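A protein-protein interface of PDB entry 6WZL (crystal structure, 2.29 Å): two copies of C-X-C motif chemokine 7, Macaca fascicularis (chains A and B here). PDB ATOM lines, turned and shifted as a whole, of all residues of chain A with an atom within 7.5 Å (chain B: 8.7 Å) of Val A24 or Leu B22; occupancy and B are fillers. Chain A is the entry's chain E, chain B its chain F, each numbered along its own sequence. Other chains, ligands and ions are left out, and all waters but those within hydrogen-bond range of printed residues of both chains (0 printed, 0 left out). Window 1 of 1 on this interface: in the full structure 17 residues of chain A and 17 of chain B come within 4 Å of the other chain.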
ATOM      1  N   LEU A  22      14.950 -14.196 -15.526  1.00  0.00           N
ATOM      2  CA  LEU A  22      14.906 -12.745 -15.424  1.00  0.00           C
ATOM      3  C   LEU A  22      15.964 -12.249 -14.506  1.00  0.00           C
ATOM      4  O   LEU A  22      16.134 -12.769 -13.396  1.00  0.00           O
ATOM      5  CB  LEU A  22      13.545 -12.268 -14.904  1.00  0.00           C
ATOM      6  CG  LEU A  22      12.458 -11.997 -15.880  1.00  0.00           C
ATOM      7  CD1 LEU A  22      11.107 -12.437 -15.306  1.00  0.00           C
ATOM      8  CD2 LEU A  22      12.425 -10.550 -16.223  1.00  0.00           C
ATOM      9  N   GLU A  23      16.677 -11.224 -14.954  1.00  0.00           N
ATOM     10  CA  GLU A  23      17.706 -10.626 -14.146  1.00  0.00           C
ATOM     11  C   GLU A  23      17.316  -9.210 -13.748  1.00  0.00           C
ATOM     12  O   GLU A  23      17.002  -8.390 -14.606  1.00  0.00           O
ATOM     13  CB  GLU A  23      19.078 -10.694 -14.824  1.00  0.00           C
ATOM     14  CG  GLU A  23      20.212 -10.625 -13.810  1.00  0.00           C
ATOM     15  CD  GLU A  23      21.627 -10.486 -14.341  1.00  0.00           C
ATOM     16  OE1 GLU A  23      21.795 -10.214 -15.552  1.00  0.00           O
ATOM     17  OE2 GLU A  23      22.571 -10.636 -13.530  1.00  0.00           O
ATOM     18  N   VAL A  24      17.315  -8.943 -12.442  1.00  0.00           N
ATOM     19  CA  VAL A  24      17.006  -7.631 -11.898  1.00  0.00           C
ATOM     20  C   VAL A  24      18.335  -7.032 -11.505  1.00  0.00           C
ATOM     21  O   VAL A  24      18.999  -7.563 -10.627  1.00  0.00           O
ATOM     22  CB  VAL A  24      16.018  -7.689 -10.704  1.00  0.00           C
ATOM     23  CG1 VAL A  24      15.686  -6.284 -10.186  1.00  0.00           C
ATOM     24  CG2 VAL A  24      14.742  -8.442 -11.078  1.00  0.00           C
ATOM     25  N   ILE A  25      18.745  -5.950 -12.172  1.00  0.00           N
ATOM     26  CA  ILE A  25      20.012  -5.308 -11.860  1.00  0.00           C
ATOM     27  C   ILE A  25      19.734  -3.961 -11.209  1.00  0.00           C
ATOM     28  O   ILE A  25      19.085  -3.106 -11.820  1.00  0.00           O
ATOM     29  CB  ILE A  25      20.935  -5.173 -13.097  1.00  0.00           C
ATOM     30  CG1 ILE A  25      21.096  -6.504 -13.825  1.00  0.00           C
ATOM     31  CG2 ILE A  25      22.284  -4.587 -12.697  1.00  0.00           C
ATOM     32  CD1 ILE A  25      20.978  -6.408 -15.315  1.00  0.00           C
ATOM     33  N   GLY A  26      20.222  -3.796  -9.979  1.00  0.00           N
ATOM     34  CA  GLY A  26      20.069  -2.545  -9.251  1.00  0.00           C
ATOM     35  C   GLY A  26      21.054  -1.512  -9.755  1.00  0.00           C
ATOM     36  O   GLY A  26      22.004  -1.860 -10.472  1.00  0.00           O
ATOM     37  N   VAL A  34      18.113   1.171 -13.228  1.00  0.00           N
ATOM     38  CA  VAL A  34      17.698  -0.162 -12.802  1.00  0.00           C
ATOM     39  C   VAL A  34      17.350  -0.868 -14.121  1.00  0.00           C
ATOM     40  O   VAL A  34      16.682  -0.275 -14.964  1.00  0.00           O
ATOM     41  CB  VAL A  34      16.503  -0.155 -11.810  1.00  0.00           C
ATOM     42  CG1 VAL A  34      16.006  -1.580 -11.537  1.00  0.00           C
ATOM     43  CG2 VAL A  34      16.885   0.524 -10.505  1.00  0.00           C
ATOM     44  N   GLU A  35      17.842  -2.099 -14.327  1.00  0.00           N
ATOM     45  CA  GLU A  35      17.590  -2.812 -15.582  1.00  0.00           C
ATOM     46  C   GLU A  35      16.996  -4.186 -15.323  1.00  0.00           C
ATOM     47  O   GLU A  35      17.398  -4.875 -14.383  1.00  0.00           O
ATOM     48  CB  GLU A  35      18.885  -2.940 -16.417  1.00  0.00           C
ATOM     49  CG  GLU A  35      19.761  -1.699 -16.374  1.00  0.00           C
ATOM     50  CD  GLU A  35      20.681  -1.449 -17.544  1.00  0.00           C
ATOM     51  OE1 GLU A  35      21.647  -2.228 -17.724  1.00  0.00           O
ATOM     52  OE2 GLU A  35      20.457  -0.443 -18.258  1.00  0.00           O
ATOM     53  N   VAL A  36      16.037  -4.580 -16.158  1.00  0.00           N
ATOM     54  CA  VAL A  36      15.404  -5.889 -16.050  1.00  0.00           C
ATOM     55  C   VAL A  36      15.562  -6.630 -17.373  1.00  0.00           C
ATOM     56  O   VAL A  36      14.950  -6.241 -18.351  1.00  0.00           O
ATOM     57  CB  VAL A  36      13.933  -5.856 -15.526  1.00  0.00           C
ATOM     58  CG1 VAL A  36      13.396  -7.281 -15.347  1.00  0.00           C
ATOM     59  CG2 VAL A  36      13.835  -5.083 -14.213  1.00  0.00           C
ATOM     60  N   ILE A  37      16.418  -7.667 -17.410  1.00  0.00           N
ATOM     61  CA  ILE A  37      16.640  -8.444 -18.630  1.00  0.00           C
ATOM     62  C   ILE A  37      16.018  -9.827 -18.505  1.00  0.00           C
ATOM     63  O   ILE A  37      16.357 -10.584 -17.606  1.00  0.00           O
ATOM     64  CB  ILE A  37      18.131  -8.487 -19.089  1.00  0.00           C
ATOM     65  CG1 ILE A  37      18.669  -7.063 -19.320  1.00  0.00           C
ATOM     66  CG2 ILE A  37      18.297  -9.367 -20.367  1.00  0.00           C
ATOM     67  CD1 ILE A  37      20.125  -6.903 -18.967  1.00  0.00           C
ATOM     68  N   ALA A  38      15.124 -10.143 -19.429  1.00  0.00           N
ATOM     69  CA  ALA A  38      14.435 -11.419 -19.513  1.00  0.00           C
ATOM     70  C   ALA A  38      15.027 -12.242 -20.628  1.00  0.00           C
ATOM     71  O   ALA A  38      15.206 -11.721 -21.729  1.00  0.00           O
ATOM     72  CB  ALA A  38      12.957 -11.180 -19.795  1.00  0.00           C
ATOM     73  N   PRO A  50      11.123  -1.658 -15.692  1.00  0.00           N
ATOM     74  CA  PRO A  50      11.300  -2.036 -14.281  1.00  0.00           C
ATOM     75  C   PRO A  50      10.220  -1.528 -13.310  1.00  0.00           C
ATOM     76  O   PRO A  50      10.542  -1.245 -12.150  1.00  0.00           O
ATOM     77  CB  PRO A  50      12.695  -1.474 -13.958  1.00  0.00           C
ATOM     78  CG  PRO A  50      12.810  -0.291 -14.819  1.00  0.00           C
ATOM     79  CD  PRO A  50      12.123  -0.648 -16.099  1.00  0.00           C
ATOM     80  N   ILE A  55       6.765  -6.262 -12.664  1.00  0.00           N
ATOM     81  CA  ILE A  55       8.045  -6.971 -12.647  1.00  0.00           C
ATOM     82  C   ILE A  55       7.997  -8.051 -11.567  1.00  0.00           C
ATOM     83  O   ILE A  55       8.530  -9.147 -11.770  1.00  0.00           O
ATOM     84  CB  ILE A  55       9.243  -6.003 -12.454  1.00  0.00           C
ATOM     85  N   LYS A  56       7.324  -7.746 -10.434  1.00  0.00           N
ATOM     86  CA  LYS A  56       7.137  -8.679  -9.322  1.00  0.00           C
ATOM     87  C   LYS A  56       6.098  -9.751  -9.673  1.00  0.00           C
ATOM     88  O   LYS A  56       6.167 -10.850  -9.117  1.00  0.00           O
ATOM     89  CB  LYS A  56       6.778  -7.944  -8.019  1.00  0.00           C
ATOM     90  CG  LYS A  56       7.914  -7.919  -6.994  1.00  0.00           C
ATOM     91  CD  LYS A  56       8.028  -6.588  -6.235  1.00  0.00           C
ATOM     92  CE  LYS A  56       6.986  -6.370  -5.151  1.00  0.00           C
ATOM     93  NZ  LYS A  56       5.814  -5.595  -5.651  1.00  0.00           N
ATOM     94  N   VAL A  59       8.089 -11.923 -11.938  1.00  0.00           N
ATOM     95  CA  VAL A  59       9.110 -12.500 -11.049  1.00  0.00           C
ATOM     96  C   VAL A  59       8.530 -13.578 -10.151  1.00  0.00           C
ATOM     97  O   VAL A  59       9.061 -14.681 -10.169  1.00  0.00           O
ATOM     98  CB  VAL A  59       9.938 -11.471 -10.246  1.00  0.00           C
ATOM     99  N   LEU A  63       9.460 -17.346  -9.855  1.00  0.00           N
ATOM    100  CA  LEU A  63       9.952 -17.552  -8.494  1.00  0.00           C
ATOM    101  C   LEU A  63       9.101 -18.574  -7.767  1.00  0.00           C
ATOM    102  O   LEU A  63       9.319 -18.775  -6.580  1.00  0.00           O
ATOM    103  CB  LEU A  63       9.933 -16.180  -7.768  1.00  0.00           C
ATOM    104  CG  LEU A  63      10.693 -15.973  -6.462  1.00  0.00           C
ATOM    105  CD1 LEU A  63      12.185 -16.136  -6.644  1.00  0.00           C
ATOM    106  CD2 LEU A  63      10.421 -14.611  -5.932  1.00  0.00           C
ATOM    107  N   PRO B  16      20.362  -6.540   1.319  1.00  0.00           N
ATOM    108  CA  PRO B  16      20.166  -6.088  -0.076  1.00  0.00           C
ATOM    109  C   PRO B  16      21.192  -5.050  -0.525  1.00  0.00           C
ATOM    110  O   PRO B  16      21.575  -5.043  -1.698  1.00  0.00           O
ATOM    111  CB  PRO B  16      18.738  -5.524  -0.077  1.00  0.00           C
ATOM    112  CG  PRO B  16      18.069  -6.186   1.067  1.00  0.00           C
ATOM    113  CD  PRO B  16      19.127  -6.370   2.109  1.00  0.00           C
ATOM    114  N   ILE B  19      23.872  -6.641  -2.518  1.00  0.00           N
ATOM    115  CA  ILE B  19      23.520  -7.293  -3.780  1.00  0.00           C
ATOM    116  C   ILE B  19      23.515  -6.302  -4.936  1.00  0.00           C
ATOM    117  O   ILE B  19      22.839  -5.278  -4.862  1.00  0.00           O
ATOM    118  CB  ILE B  19      22.175  -8.083  -3.684  1.00  0.00           C
ATOM    119  CG1 ILE B  19      22.175  -9.071  -2.501  1.00  0.00           C
ATOM    120  CG2 ILE B  19      21.845  -8.808  -5.012  1.00  0.00           C
ATOM    121  CD1 ILE B  19      20.739  -9.389  -1.961  1.00  0.00           C
ATOM    122  N   GLN B  20      24.252  -6.615  -6.010  1.00  0.00           N
ATOM    123  CA  GLN B  20      24.243  -5.793  -7.217  1.00  0.00           C
ATOM    124  C   GLN B  20      23.045  -6.211  -8.107  1.00  0.00           C
ATOM    125  O   GLN B  20      22.259  -5.359  -8.515  1.00  0.00           O
ATOM    126  CB  GLN B  20      25.579  -5.888  -7.984  1.00  0.00           C
ATOM    127  CG  GLN B  20      25.655  -4.928  -9.182  1.00  0.00           C
ATOM    128  CD  GLN B  20      25.379  -3.476  -8.835  1.00  0.00           C
ATOM    129  OE1 GLN B  20      25.996  -2.896  -7.941  1.00  0.00           O
ATOM    130  NE2 GLN B  20      24.437  -2.860  -9.525  1.00  0.00           N
ATOM    131  N   SER B  21      22.909  -7.524  -8.381  1.00  0.00           N
ATOM    132  CA  SER B  21      21.864  -8.068  -9.241  1.00  0.00           C
ATOM    133  C   SER B  21      21.384  -9.442  -8.790  1.00  0.00           C
ATOM    134  O   SER B  21      22.049 -10.116  -8.002  1.00  0.00           O
ATOM    135  CB  SER B  21      22.356  -8.136 -10.685  1.00  0.00           C
ATOM    136  OG  SER B  21      23.458  -9.020 -10.807  1.00  0.00           O
ATOM    137  N   LEU B  22      20.248  -9.871  -9.324  1.00  0.00           N
ATOM    138  CA  LEU B  22      19.662 -11.148  -8.985  1.00  0.00           C
ATOM    139  C   LEU B  22      19.023 -11.780 -10.181  1.00  0.00           C
ATOM    140  O   LEU B  22      18.282 -11.121 -10.908  1.00  0.00           O
ATOM    141  CB  LEU B  22      18.705 -11.084  -7.761  1.00  0.00           C
ATOM    142  CG  LEU B  22      17.483 -10.179  -7.670  1.00  0.00           C
ATOM    143  CD1 LEU B  22      16.632 -10.627  -6.498  1.00  0.00           C
ATOM    144  CD2 LEU B  22      17.843  -8.693  -7.502  1.00  0.00           C
ATOM    145  N   GLU B  23      19.330 -13.057 -10.401  1.00  0.00           N
ATOM    146  CA  GLU B  23      18.746 -13.780 -11.502  1.00  0.00           C
ATOM    147  C   GLU B  23      17.802 -14.854 -10.973  1.00  0.00           C
ATOM    148  O   GLU B  23      18.185 -15.669 -10.131  1.00  0.00           O
ATOM    149  CB  GLU B  23      19.824 -14.360 -12.423  1.00  0.00           C
ATOM    150  CG  GLU B  23      19.303 -14.619 -13.828  1.00  0.00           C
ATOM    151  CD  GLU B  23      20.233 -15.346 -14.781  1.00  0.00           C
ATOM    152  OE1 GLU B  23      21.259 -15.910 -14.332  1.00  0.00           O
ATOM    153  OE2 GLU B  23      19.923 -15.355 -15.995  1.00  0.00           O
ATOM    154  N   VAL B  24      16.564 -14.832 -11.455  1.00  0.00           N
ATOM    155  CA  VAL B  24      15.553 -15.805 -11.098  1.00  0.00           C
ATOM    156  C   VAL B  24      15.451 -16.749 -12.287  1.00  0.00           C
ATOM    157  O   VAL B  24      15.091 -16.322 -13.383  1.00  0.00           O
ATOM    158  CB  VAL B  24      14.181 -15.141 -10.773  1.00  0.00           C
ATOM    159  CG1 VAL B  24      13.150 -16.195 -10.370  1.00  0.00           C
ATOM    160  CG2 VAL B  24      14.326 -14.069  -9.693  1.00  0.00           C
ATOM    161  N   ILE B  25      15.800 -18.014 -12.086  1.00  0.00           N
ATOM    162  CA  ILE B  25      15.749 -18.989 -13.165  1.00  0.00           C
ATOM    163  C   ILE B  25      14.639 -19.977 -12.896  1.00  0.00           C
ATOM    164  O   ILE B  25      14.647 -20.643 -11.855  1.00  0.00           O
ATOM    165  CB  ILE B  25      17.119 -19.701 -13.377  1.00  0.00           C
ATOM    166  CG1 ILE B  25      18.249 -18.679 -13.547  1.00  0.00           C
ATOM    167  CG2 ILE B  25      17.058 -20.666 -14.575  1.00  0.00           C
ATOM    168  CD1 ILE B  25      19.470 -19.053 -12.797  1.00  0.00           C
ATOM    169  N   GLU B  35      16.041 -21.596  -9.400  1.00  0.00           N
ATOM    170  CA  GLU B  35      17.314 -21.157  -8.833  1.00  0.00           C
ATOM    171  C   GLU B  35      17.384 -19.637  -8.767  1.00  0.00           C
ATOM    172  O   GLU B  35      16.927 -18.948  -9.689  1.00  0.00           O
ATOM    173  CB  GLU B  35      18.511 -21.712  -9.651  1.00  0.00           C
ATOM    174  CG  GLU B  35      18.337 -23.171 -10.068  1.00  0.00           C
ATOM    175  CD  GLU B  35      19.581 -23.999 -10.334  1.00  0.00           C
ATOM    176  OE1 GLU B  35      19.804 -24.987  -9.600  1.00  0.00           O
ATOM    177  OE2 GLU B  35      20.320 -23.677 -11.293  1.00  0.00           O
ATOM    178  N   VAL B  36      17.960 -19.116  -7.672  1.00  0.00           N
ATOM    179  CA  VAL B  36      18.117 -17.679  -7.507  1.00  0.00           C
ATOM    180  C   VAL B  36      19.596 -17.353  -7.292  1.00  0.00           C
ATOM    181  O   VAL B  36      20.141 -17.694  -6.250  1.00  0.00           O
ATOM    182  CB  VAL B  36      17.177 -17.045  -6.444  1.00  0.00           C
ATOM    183  CG1 VAL B  36      17.332 -15.525  -6.417  1.00  0.00           C
ATOM    184  CG2 VAL B  36      15.724 -17.406  -6.719  1.00  0.00           C
ATOM    185  N   ILE B  37      20.247 -16.725  -8.295  1.00  0.00           N
ATOM    186  CA  ILE B  37      21.656 -16.366  -8.180  1.00  0.00           C
ATOM    187  C   ILE B  37      21.815 -14.865  -8.034  1.00  0.00           C
ATOM    188  O   ILE B  37      21.386 -14.106  -8.897  1.00  0.00           O
ATOM    189  CB  ILE B  37      22.556 -16.968  -9.293  1.00  0.00           C
ATOM    190  CG1 ILE B  37      22.468 -18.518  -9.299  1.00  0.00           C
ATOM    191  CG2 ILE B  37      24.036 -16.504  -9.134  1.00  0.00           C
ATOM    192  CD1 ILE B  37      22.562 -19.182 -10.670  1.00  0.00           C
ATOM    193  N   ALA B  38      22.441 -14.448  -6.928  1.00  0.00           N
ATOM    194  CA  ALA B  38      22.724 -13.055  -6.607  1.00  0.00           C
ATOM    195  C   ALA B  38      24.175 -12.760  -6.877  1.00  0.00           C
ATOM    196  O   ALA B  38      25.038 -13.532  -6.459  1.00  0.00           O
ATOM    197  CB  ALA B  38      22.426 -12.778  -5.135  1.00  0.00           C
ATOM    198  N   THR B  39      24.457 -11.638  -7.566  1.00  0.00           N
ATOM    199  CA  THR B  39      25.828 -11.166  -7.782  1.00  0.00           C
ATOM    200  C   THR B  39      26.021 -10.077  -6.747  1.00  0.00           C
ATOM    201  O   THR B  39      25.223  -9.143  -6.653  1.00  0.00           O
ATOM    202  CB  THR B  39      26.066 -10.678  -9.211  1.00  0.00           C
ATOM    203  OG1 THR B  39      25.677 -11.695 -10.127  1.00  0.00           O
ATOM    204  CG2 THR B  39      27.518 -10.343  -9.457  1.00  0.00           C
ATOM    205  N   LEU B  40      27.026 -10.238  -5.925  1.00  0.00           N
ATOM    206  CA  LEU B  40      27.281  -9.294  -4.859  1.00  0.00           C
ATOM    207  C   LEU B  40      28.094  -8.113  -5.366  1.00  0.00           C
ATOM    208  O   LEU B  40      28.650  -8.177  -6.467  1.00  0.00           O
ATOM    209  CB  LEU B  40      27.939  -9.977  -3.643  1.00  0.00           C
ATOM    210  CG  LEU B  40      27.240 -11.229  -3.096  1.00  0.00           C
ATOM    211  CD1 LEU B  40      28.092 -11.893  -2.035  1.00  0.00           C
ATOM    212  CD2 LEU B  40      25.806 -10.908  -2.569  1.00  0.00           C
ATOM    213  N   ILE B  46      26.276 -15.934  -5.679  1.00  0.00           N
ATOM    214  CA  ILE B  46      25.773 -16.693  -4.540  1.00  0.00           C
ATOM    215  C   ILE B  46      24.324 -17.165  -4.768  1.00  0.00           C
ATOM    216  O   ILE B  46      23.512 -16.403  -5.287  1.00  0.00           O
ATOM    217  CB  ILE B  46      25.995 -15.791  -3.263  1.00  0.00           C
ATOM    218  CG1 ILE B  46      26.369 -16.603  -2.049  1.00  0.00           C
ATOM    219  CG2 ILE B  46      24.854 -14.805  -2.933  1.00  0.00           C
ATOM    220  CD1 ILE B  46      27.500 -15.971  -1.270  1.00  0.00           C
ATOM    221  N   LEU B  48      20.664 -18.202  -3.581  1.00  0.00           N
ATOM    222  CA  LEU B  48      19.752 -17.801  -2.516  1.00  0.00           C
ATOM    223  C   LEU B  48      18.540 -18.715  -2.480  1.00  0.00           C
ATOM    224  O   LEU B  48      18.152 -19.288  -3.510  1.00  0.00           O
ATOM    225  CB  LEU B  48      19.294 -16.347  -2.679  1.00  0.00           C
ATOM    226  CG  LEU B  48      20.353 -15.235  -2.797  1.00  0.00           C
ATOM    227  CD1 LEU B  48      19.686 -13.908  -2.893  1.00  0.00           C
ATOM    228  CD2 LEU B  48      21.312 -15.208  -1.616  1.00  0.00           C
ATOM    229  N   ARG B  54      10.873 -13.300   0.579  1.00  0.00           N
ATOM    230  CA  ARG B  54      12.227 -12.753   0.761  1.00  0.00           C
ATOM    231  C   ARG B  54      12.851 -12.200  -0.548  1.00  0.00           C
ATOM    232  O   ARG B  54      13.349 -11.071  -0.564  1.00  0.00           O
ATOM    233  CB  ARG B  54      13.144 -13.771   1.447  1.00  0.00           C
ATOM    234  N   ILE B  55      12.765 -12.964  -1.648  1.00  0.00           N
ATOM    235  CA  ILE B  55      13.288 -12.515  -2.941  1.00  0.00           C
ATOM    236  C   ILE B  55      12.473 -11.312  -3.493  1.00  0.00           C
ATOM    237  O   ILE B  55      13.061 -10.432  -4.124  1.00  0.00           O
ATOM    238  CB  ILE B  55      13.439 -13.677  -3.960  1.00  0.00           C
ATOM    239  N   LYS B  56      11.141 -11.254  -3.210  1.00  0.00           N
ATOM    240  CA  LYS B  56      10.261 -10.148  -3.635  1.00  0.00           C
ATOM    241  C   LYS B  56      10.539  -8.846  -2.867  1.00  0.00           C
ATOM    242  O   LYS B  56      10.287  -7.771  -3.407  1.00  0.00           O
ATOM    243  CB  LYS B  56       8.771 -10.532  -3.596  1.00  0.00           C
ATOM    244  CG  LYS B  56       8.285 -11.136  -4.916  1.00  0.00           C
ATOM    245  CD  LYS B  56       6.853 -11.643  -4.846  1.00  0.00           C
ATOM    246  N   LYS B  57      11.087  -8.943  -1.633  1.00  0.00           N
ATOM    247  CA  LYS B  57      11.477  -7.781  -0.827  1.00  0.00           C
ATOM    248  C   LYS B  57      12.752  -7.138  -1.436  1.00  0.00           C
ATOM    249  O   LYS B  57      12.787  -5.920  -1.637  1.00  0.00           O
ATOM    250  CB  LYS B  57      11.707  -8.183   0.635  1.00  0.00           C
ATOM    251  N   ILE B  58      13.775  -7.973  -1.765  1.00  0.00           N
ATOM    252  CA  ILE B  58      15.016  -7.556  -2.421  1.00  0.00           C
ATOM    253  C   ILE B  58      14.678  -6.960  -3.798  1.00  0.00           C
ATOM    254  O   ILE B  58      15.165  -5.883  -4.114  1.00  0.00           O
ATOM    255  CB  ILE B  58      16.034  -8.723  -2.528  1.00  0.00           C
ATOM    256  N   VAL B  59      13.785  -7.615  -4.568  1.00  0.00           N
ATOM    257  CA  VAL B  59      13.363  -7.170  -5.897  1.00  0.00           C
ATOM    258  C   VAL B  59      12.711  -5.786  -5.888  1.00  0.00           C
ATOM    259  O   VAL B  59      13.074  -4.973  -6.730  1.00  0.00           O
ATOM    260  CB  VAL B  59      12.479  -8.206  -6.625  1.00  0.00           C
ATOM    261  N   GLN B  60      11.787  -5.499  -4.939  1.00  0.00           N
ATOM    262  CA  GLN B  60      11.116  -4.191  -4.824  1.00  0.00           C
ATOM    263  C   GLN B  60      12.128  -3.111  -4.405  1.00  0.00           C
ATOM    264  O   GLN B  60      12.130  -2.008  -4.972  1.00  0.00           O
ATOM    265  CB  GLN B  60       9.897  -4.284  -3.869  1.00  0.00           C
ATOM    266  CG  GLN B  60       9.475  -3.007  -3.100  1.00  0.00           C
ATOM    267  CD  GLN B  60       8.780  -1.939  -3.920  1.00  0.00           C
ATOM    268  OE1 GLN B  60       7.829  -2.203  -4.667  1.00  0.00           O
ATOM    269  NE2 GLN B  60       9.217  -0.691  -3.764  1.00  0.00           N
ATOM    270  N   LYS B  61      13.014  -3.452  -3.446  1.00  0.00           N
ATOM    271  CA  LYS B  61      14.057  -2.555  -2.960  1.00  0.00           C
ATOM    272  C   LYS B  61      15.077  -2.219  -4.072  1.00  0.00           C
ATOM    273  O   LYS B  61      15.656  -1.131  -4.054  1.00  0.00           O
ATOM    274  CB  LYS B  61      14.742  -3.140  -1.712  1.00  0.00           C
ATOM    275  N   LYS B  62      15.276  -3.132  -5.043  1.00  0.00           N
ATOM    276  CA  LYS B  62      16.189  -2.891  -6.162  1.00  0.00           C
ATOM    277  C   LYS B  62      15.568  -1.930  -7.199  1.00  0.00           C
ATOM    278  O   LYS B  62      16.274  -1.056  -7.712  1.00  0.00           O
ATOM    279  CB  LYS B  62      16.663  -4.209  -6.818  1.00  0.00           C
ATOM    280  CG  LYS B  62      17.677  -5.017  -5.990  1.00  0.00           C
ATOM    281  CD  LYS B  62      19.086  -4.428  -5.981  1.00  0.00           C
ATOM    282  CE  LYS B  62      19.611  -4.250  -4.580  1.00  0.00           C
ATOM    283  NZ  LYS B  62      20.821  -3.384  -4.556  1.00  0.00           N
ATOM    284  N   LEU B  63      14.249  -2.071  -7.469  1.00  0.00           N
ATOM    285  CA  LEU B  63      13.514  -1.225  -8.426  1.00  0.00           C
ATOM    286  C   LEU B  63      13.149   0.169  -7.849  1.00  0.00           C
ATOM    287  O   LEU B  63      12.772   1.061  -8.612  1.00  0.00           O
ATOM    288  CB  LEU B  63      12.270  -1.949  -9.005  1.00  0.00           C
ATOM    289  CG  LEU B  63      12.469  -3.398  -9.508  1.00  0.00           C
ATOM    290  CD1 LEU B  63      11.231  -4.216  -9.347  1.00  0.00           C
ATOM    291  CD2 LEU B  63      12.878  -3.450 -10.940  1.00  0.00           C
ATOM    292  N   ALA B  64      13.298   0.366  -6.518  1.00  0.00           N
ATOM    293  CA  ALA B  64      13.010   1.638  -5.842  1.00  0.00           C
ATOM    294  C   ALA B  64      14.251   2.242  -5.159  1.00  0.00           C
ATOM    295  O   ALA B  64      14.539   1.990  -3.985  1.00  0.00           O
ATOM    296  CB  ALA B  64      11.868   1.464  -4.848  1.00  0.00           C
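O of Leu A22 touches O of Leu B22, at 3.7 Å.
Leu A22 touches Glu B23 (O to CA, 3.4 Å).
Glu A23 touches Leu B22 (CA to O, 3.3 Å).
Ser B21 touches Val A24 (CA to O, 3.2 Å).
Gly A26 touches Lys B62 (CA to CD, 3.9 Å).
Val A34 touches Lys B62.
CD2 of Leu B63 touches O of Pro A50 (3.4 Å).
Lys A56 touches Lys B56 (CD to O, 3.8 Å).
Gln B60 touches Lys A56.
CG2 of Val B36 touches CD1 of Leu A63, 3.8 Å away.
Of chain B, only Ser B21 (3.2 Å) and Leu B22 (2.8 Å) come within 4 Å of Val A24.
Leu B22 touches three residues of chain A.
Printed residues of chain A within 4 Å of Lys B62: Gly A26 and Val A34.
Printed residues of chain B within 4 Å of Leu A22: Leu B22, Glu B23 and Val B24.
Printed residues of chain A within 4 Å of Ser B21: Glu A23, Val A24 and Ile A25.
Printed residues of chain A within 4 Å of Ile B55: Leu A63 (3.7 Å).
Printed residues of chain B within 4 Å of Ile A25: Gln B20 (3.9 Å) and Ser B21 (3.8 Å).
Val B59 touches none of the printed residues of chain A.
The backbone carbonyl oxygen (O) of Pro B16 lies within hydrogen-bond range of the side-chain amino group (NZ) of Lys B62 (3.4 Å).
N of Thr B39 is in hydrogen-bond range of O of Ser B21, 2.9 Å away.
O of Val B36 lies within hydrogen-bond range of N of Leu B48 (2.8 Å).
N of Glu A23 lies within hydrogen-bond range of O of Ile A37 (2.7 Å).
The backbone NH (N) of Gln B20 lies within hydrogen-bond range of the backbone carbonyl oxygen (O) of Thr B39.
O of Ile B19 lies within hydrogen-bond range of NZ of Lys B62 (2.8 Å).
Leu A22 touches Val B24, and with the chains exchanged Val A24 touches Leu B22.
Val A36 touches Leu B63, and with the chains exchanged Leu A63 touches Val B36.
Lys A56 touches its own counterpart, Lys B56.
Leu A63 touches Ile B55, but with the chains exchanged Ile A55 does not touch Leu B63 (4.1 Å).
12 positions are printed for both chains.
O of Gly A26 lies within hydrogen-bond range of NE2 of Gln B20 (2.8 Å).
The backbone NH (N) of Val A24 is in hydrogen-bond range of the backbone carbonyl oxygen (O) of Leu B22 (2.8 Å).
O of Leu A22 sits at hydrogen-bond distance from N of Val B24.
The side-chain carboxylate (OE2) of Glu A23 is in hydrogen-bond range of the side-chain hydroxyl (OG) of Ser B21, 3.3 Å away.
Hydrophobic or aromatic side chains of chain B within 4 Å of the printed part of chain A: Leu B22, Val B24, Val B36, Ile B55 and Leu B63.
Of the 15 printed residues of chain A, 10 touch a printed residue of chain B.
Hydrophobic or aromatic side chains of chain A within 4 Å of the printed part of chain B: Val A24, Ile A25, Val A34, Val A36, Pro A50 and Leu A63.
Among the printed residues, 20 pairs touch across the chains.
Among the printed residues, no Asp or Glu carboxylate lies within 4 Å of a Lys or Arg side-chain nitrogen of the other chain.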
